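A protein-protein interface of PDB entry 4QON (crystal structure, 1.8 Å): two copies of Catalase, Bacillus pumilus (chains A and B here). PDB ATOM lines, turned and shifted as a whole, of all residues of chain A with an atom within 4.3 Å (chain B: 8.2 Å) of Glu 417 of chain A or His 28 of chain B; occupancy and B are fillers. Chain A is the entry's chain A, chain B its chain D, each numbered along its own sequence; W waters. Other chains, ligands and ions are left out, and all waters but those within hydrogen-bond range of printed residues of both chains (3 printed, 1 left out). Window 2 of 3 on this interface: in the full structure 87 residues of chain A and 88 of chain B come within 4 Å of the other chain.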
ATOM      1  N   LYS A 331      28.616  -5.108  23.777  1.00  0.00           N
ATOM      2  CA  LYS A 331      28.646  -3.648  24.052  1.00  0.00           C
ATOM      3  C   LYS A 331      30.091  -3.142  24.292  1.00  0.00           C
ATOM      4  O   LYS A 331      30.367  -1.955  24.132  1.00  0.00           O
ATOM      5  CB  LYS A 331      27.797  -3.292  25.279  1.00  0.00           C
ATOM      6  CG  LYS A 331      26.329  -3.601  25.098  1.00  0.00           C
ATOM      7  CD  LYS A 331      25.516  -3.101  26.268  1.00  0.00           C
ATOM      8  CE  LYS A 331      24.108  -3.741  26.264  1.00  0.00           C
ATOM      9  NZ  LYS A 331      23.406  -3.315  27.480  1.00  0.00           N
ATOM     10  N   GLN A 414      20.715  -0.029  29.843  1.00  0.00           N
ATOM     11  CA  GLN A 414      20.296  -1.145  30.682  1.00  0.00           C
ATOM     12  C   GLN A 414      21.251  -2.328  30.530  1.00  0.00           C
ATOM     13  O   GLN A 414      21.594  -2.690  29.428  1.00  0.00           O
ATOM     14  CB  GLN A 414      18.899  -1.541  30.227  1.00  0.00           C
ATOM     15  CG  GLN A 414      18.129  -2.518  31.070  1.00  0.00           C
ATOM     16  CD  GLN A 414      16.851  -2.885  30.348  1.00  0.00           C
ATOM     17  OE1 GLN A 414      16.283  -2.057  29.641  1.00  0.00           O
ATOM     18  NE2 GLN A 414      16.413  -4.129  30.491  1.00  0.00           N
ATOM     19  N   LYS A 415      21.655  -2.932  31.635  1.00  0.00           N
ATOM     20  CA  LYS A 415      22.473  -4.157  31.607  1.00  0.00           C
ATOM     21  C   LYS A 415      21.811  -5.284  30.800  1.00  0.00           C
ATOM     22  O   LYS A 415      20.576  -5.389  30.739  1.00  0.00           O
ATOM     23  CB  LYS A 415      22.751  -4.635  33.037  1.00  0.00           C
ATOM     24  CG  LYS A 415      23.781  -5.751  33.143  1.00  0.00           C
ATOM     25  CD  LYS A 415      23.866  -6.320  34.560  1.00  0.00           C
ATOM     26  CE  LYS A 415      24.345  -5.302  35.581  1.00  0.00           C
ATOM     27  NZ  LYS A 415      24.482  -5.974  36.910  1.00  0.00           N
ATOM     28  N   ILE A 416      22.635  -6.114  30.152  1.00  0.00           N
ATOM     29  CA  ILE A 416      22.112  -7.280  29.469  1.00  0.00           C
ATOM     30  C   ILE A 416      21.368  -8.167  30.477  1.00  0.00           C
ATOM     31  O   ILE A 416      21.699  -8.203  31.697  1.00  0.00           O
ATOM     32  CB  ILE A 416      23.212  -8.143  28.811  1.00  0.00           C
ATOM     33  CG1 ILE A 416      24.298  -8.497  29.836  1.00  0.00           C
ATOM     34  CG2 ILE A 416      23.864  -7.444  27.639  1.00  0.00           C
ATOM     35  CD1 ILE A 416      25.138  -9.661  29.402  1.00  0.00           C
ATOM     36  N   GLU A 417      20.416  -8.936  29.951  1.00  0.00           N
ATOM     37  CA  GLU A 417      19.809 -10.049  30.694  1.00  0.00           C
ATOM     38  C   GLU A 417      20.795 -11.218  30.830  1.00  0.00           C
ATOM     39  O   GLU A 417      21.805 -11.266  30.119  1.00  0.00           O
ATOM     40  CB  GLU A 417      18.530 -10.527  29.997  1.00  0.00           C
ATOM     41  CG  GLU A 417      17.543  -9.415  29.695  1.00  0.00           C
ATOM     42  CD  GLU A 417      16.599  -9.109  30.822  1.00  0.00           C
ATOM     43  OE1 GLU A 417      15.487  -8.625  30.501  1.00  0.00           O
ATOM     44  OE2 GLU A 417      17.001  -9.294  32.003  1.00  0.00           O
ATOM     45  N   LYS A 418      20.483 -12.157  31.718  1.00  0.00           N
ATOM     46  CA  LYS A 418      21.407 -13.236  32.138  1.00  0.00           C
ATOM     47  C   LYS A 418      22.900 -12.847  32.271  1.00  0.00           C
ATOM     48  O   LYS A 418      23.762 -13.511  31.719  1.00  0.00           O
ATOM     49  CB  LYS A 418      21.334 -14.446  31.226  1.00  0.00           C
ATOM     50  CG  LYS A 418      20.374 -14.405  30.072  1.00  0.00           C
ATOM     51  CD  LYS A 418      20.405 -15.699  29.264  1.00  0.00           C
ATOM     52  CE  LYS A 418      20.424 -15.382  27.769  1.00  0.00           C
ATOM     53  NZ  LYS A 418      20.387 -16.655  26.997  1.00  0.00           N
ATOM     54  N   PRO A 419      23.207 -11.835  33.080  1.00  0.00           N
ATOM     55  CA  PRO A 419      24.634 -11.540  33.352  1.00  0.00           C
ATOM     56  C   PRO A 419      25.422 -12.753  33.896  1.00  0.00           C
ATOM     57  O   PRO A 419      26.600 -12.940  33.562  1.00  0.00           O
ATOM     58  CB  PRO A 419      24.565 -10.396  34.385  1.00  0.00           C
ATOM     59  CG  PRO A 419      23.153 -10.434  34.912  1.00  0.00           C
ATOM     60  CD  PRO A 419      22.288 -10.963  33.832  1.00  0.00           C
ATOM     61  N   ASN B  22      26.024   2.023  31.760  1.00  0.00           N
ATOM     62  CA  ASN B  22      25.529   1.422  30.538  1.00  0.00           C
ATOM     63  C   ASN B  22      25.633   2.372  29.372  1.00  0.00           C
ATOM     64  O   ASN B  22      25.141   3.506  29.439  1.00  0.00           O
ATOM     65  CB  ASN B  22      24.093   0.926  30.706  1.00  0.00           C
ATOM     66  CG  ASN B  22      23.930   0.049  31.913  1.00  0.00           C
ATOM     67  OD1 ASN B  22      24.427  -1.098  31.947  1.00  0.00           O
ATOM     68  ND2 ASN B  22      23.290   0.593  32.944  1.00  0.00           N
ATOM     69  N   SER B  23      26.179   1.873  28.276  1.00  0.00           N
ATOM     70  CA  SER B  23      26.001   2.504  26.965  1.00  0.00           C
ATOM     71  C   SER B  23      24.560   2.540  26.519  1.00  0.00           C
ATOM     72  O   SER B  23      23.761   1.703  26.900  1.00  0.00           O
ATOM     73  CB  SER B  23      26.824   1.769  25.918  1.00  0.00           C
ATOM     74  OG  SER B  23      28.170   1.989  26.186  1.00  0.00           O
ATOM     75  N   THR B  25      21.779   1.709  23.873  1.00  0.00           N
ATOM     76  CA  THR B  25      21.718   0.576  22.940  1.00  0.00           C
ATOM     77  C   THR B  25      20.279   0.288  22.472  1.00  0.00           C
ATOM     78  O   THR B  25      19.317   0.835  23.026  1.00  0.00           O
ATOM     79  CB  THR B  25      22.291  -0.690  23.566  1.00  0.00           C
ATOM     80  OG1 THR B  25      21.572  -0.989  24.782  1.00  0.00           O
ATOM     81  CG2 THR B  25      23.748  -0.527  23.867  1.00  0.00           C
ATOM     82  N   ALA B  26      20.159  -0.505  21.406  1.00  0.00           N
ATOM     83  CA  ALA B  26      18.871  -0.946  20.917  1.00  0.00           C
ATOM     84  C   ALA B  26      18.350  -2.096  21.788  1.00  0.00           C
ATOM     85  O   ALA B  26      18.565  -3.267  21.452  1.00  0.00           O
ATOM     86  CB  ALA B  26      18.967  -1.345  19.434  1.00  0.00           C
ATOM     87  N   GLY B  27      17.645  -1.739  22.866  1.00  0.00           N
ATOM     88  CA  GLY B  27      17.264  -2.670  23.914  1.00  0.00           C
ATOM     89  C   GLY B  27      18.467  -3.096  24.745  1.00  0.00           C
ATOM     90  O   GLY B  27      19.574  -2.625  24.513  1.00  0.00           O
ATOM     91  N   HIS B  28      18.248  -4.003  25.689  1.00  0.00           N
ATOM     92  CA  HIS B  28      19.253  -4.350  26.668  1.00  0.00           C
ATOM     93  C   HIS B  28      20.434  -5.116  26.049  1.00  0.00           C
ATOM     94  O   HIS B  28      21.501  -5.181  26.660  1.00  0.00           O
ATOM     95  CB  HIS B  28      18.650  -5.142  27.845  1.00  0.00           C
ATOM     96  CG  HIS B  28      17.843  -6.335  27.428  1.00  0.00           C
ATOM     97  ND1 HIS B  28      16.707  -6.726  28.104  1.00  0.00           N
ATOM     98  CD2 HIS B  28      17.967  -7.184  26.378  1.00  0.00           C
ATOM     99  CE1 HIS B  28      16.189  -7.787  27.509  1.00  0.00           C
ATOM    100  NE2 HIS B  28      16.941  -8.093  26.467  1.00  0.00           N
ATOM    101  N   ARG B  29      20.249  -5.689  24.862  1.00  0.00           N
ATOM    102  CA  ARG B  29      21.333  -6.470  24.275  1.00  0.00           C
ATOM    103  C   ARG B  29      21.716  -6.100  22.862  1.00  0.00           C
ATOM    104  O   ARG B  29      22.497  -6.802  22.241  1.00  0.00           O
ATOM    105  CB  ARG B  29      21.054  -7.980  24.381  1.00  0.00           C
ATOM    106  CG  ARG B  29      19.932  -8.480  23.488  1.00  0.00           C
ATOM    107  CD  ARG B  29      19.410  -9.849  23.883  1.00  0.00           C
ATOM    108  NE  ARG B  29      18.846 -10.601  22.768  1.00  0.00           N
ATOM    109  CZ  ARG B  29      19.568 -11.215  21.832  1.00  0.00           C
ATOM    110  NH1 ARG B  29      20.902 -11.131  21.841  1.00  0.00           N
ATOM    111  NH2 ARG B  29      18.948 -11.908  20.879  1.00  0.00           N
ATOM    112  N   GLY B  30      21.226  -4.985  22.349  1.00  0.00           N
ATOM    113  CA  GLY B  30      21.412  -4.658  20.919  1.00  0.00           C
ATOM    114  C   GLY B  30      22.689  -3.839  20.759  1.00  0.00           C
ATOM    115  O   GLY B  30      23.370  -3.557  21.750  1.00  0.00           O
ATOM    116  N   PRO B  31      23.019  -3.463  19.527  1.00  0.00           N
ATOM    117  CA  PRO B  31      24.155  -2.581  19.263  1.00  0.00           C
ATOM    118  C   PRO B  31      23.981  -1.146  19.788  1.00  0.00           C
ATOM    119  O   PRO B  31      22.868  -0.731  20.162  1.00  0.00           O
ATOM    120  CB  PRO B  31      24.274  -2.596  17.747  1.00  0.00           C
ATOM    121  CG  PRO B  31      22.966  -3.046  17.232  1.00  0.00           C
ATOM    122  CD  PRO B  31      22.287  -3.829  18.304  1.00  0.00           C
HETATM  123  O   HOH W   1      28.960   0.675  23.745  1.00  0.00           O
HETATM  124  O   HOH W   2      22.322  -0.562  27.349  1.00  0.00           O
HETATM  125  O   HOH W   3      25.383  -2.279  29.701  1.00  0.00           O
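No position is printed for both chains.
NZ of Lys 331 of chain A lies within hydrogen-bond range of O of Gln 414 of chain A (2.7 Å). The backbone carbonyl oxygen of Gly 27 of chain B sits at hydrogen-bond distance from the side-chain hydroxyl of Thr 25 of chain B (2.6 Å).
NZ of Lys 331 of chain A lies within hydrogen-bond range of O of His 28 of chain B (2.8 Å). N of Lys 415 of chain A lies within hydrogen-bond range of OD1 of Asn 22 of chain B, 3.3 Å away. The side-chain carboxylate (OE1) of Glu 417 of chain A lies close to a ring nitrogen (ND1) of His 28 of chain B (3.3 Å).
Water W2 lies within hydrogen-bond range of OG1 of Thr 25 of chain B (2.7 Å), O of Ser 23 of chain B (2.7 Å), NZ of Lys 331 of chain A (3.0 Å) and N of Gln 414 of chain A (3.0 Å). Water W3 bridges OD1 of Asn 22 of chain B (2.7 Å) and NZ of Lys 331 of chain A (3.1 Å). Water W1 bridges the side-chain hydroxyl of Ser 23 of chain B (2.9 Å) and the backbone carbonyl oxygen of Lys 331 of chain A (3.0 Å).
Printed residues of chain B within 4 Å of Glu 417 of chain A: His 28. Of the printed residues of chain A, His 28 of chain B touches Lys 331 (2.8 Å), Gln 414 (3.5 Å), Lys 415 (3.5 Å), Ile 416 (3.4 Å) and Glu 417 (3.0 Å). Printed residues of chain B within 4 Å of Lys 415 of chain A: Asn 22 (3.3 Å) and His 28 (3.5 Å). Of the printed residues of chain B, Lys 331 of chain A touches Thr 25 and His 28. Printed residues of chain B within 4 Å of Gln 414 of chain A: Asn 22 (3.6 Å) and His 28 (3.5 Å). Arg 29 of chain B touches none of the printed residues of chain A. Lys 418 of chain A touches none of the printed residues of chain B. The nearest residue of chain B that does not touch Glu 417 of chain A is Arg 29 of chain B (5.7 Å).
Thr 25 of chain B touches Lys 331 of chain A. Gln 414 of chain A touches Asn 22 of chain B (N to CB, 3.6 Å). Gln 414 of chain A touches His 28 of chain B (NE2 to ND1, 3.5 Å). CB of His 28 of chain B touches O of Lys 415 of chain A, at 3.5 Å. O of His 28 of chain B touches CG2 of Ile 416 of chain A (3.4 Å).
Printed residues of chain A that touch a printed residue of chain B: Lys 331, Gln 414, Lys 415, Ile 416 and Glu 417. Hydrophobic or aromatic side chains of chain A within 4 Å of the printed part of chain B: Ile 416.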
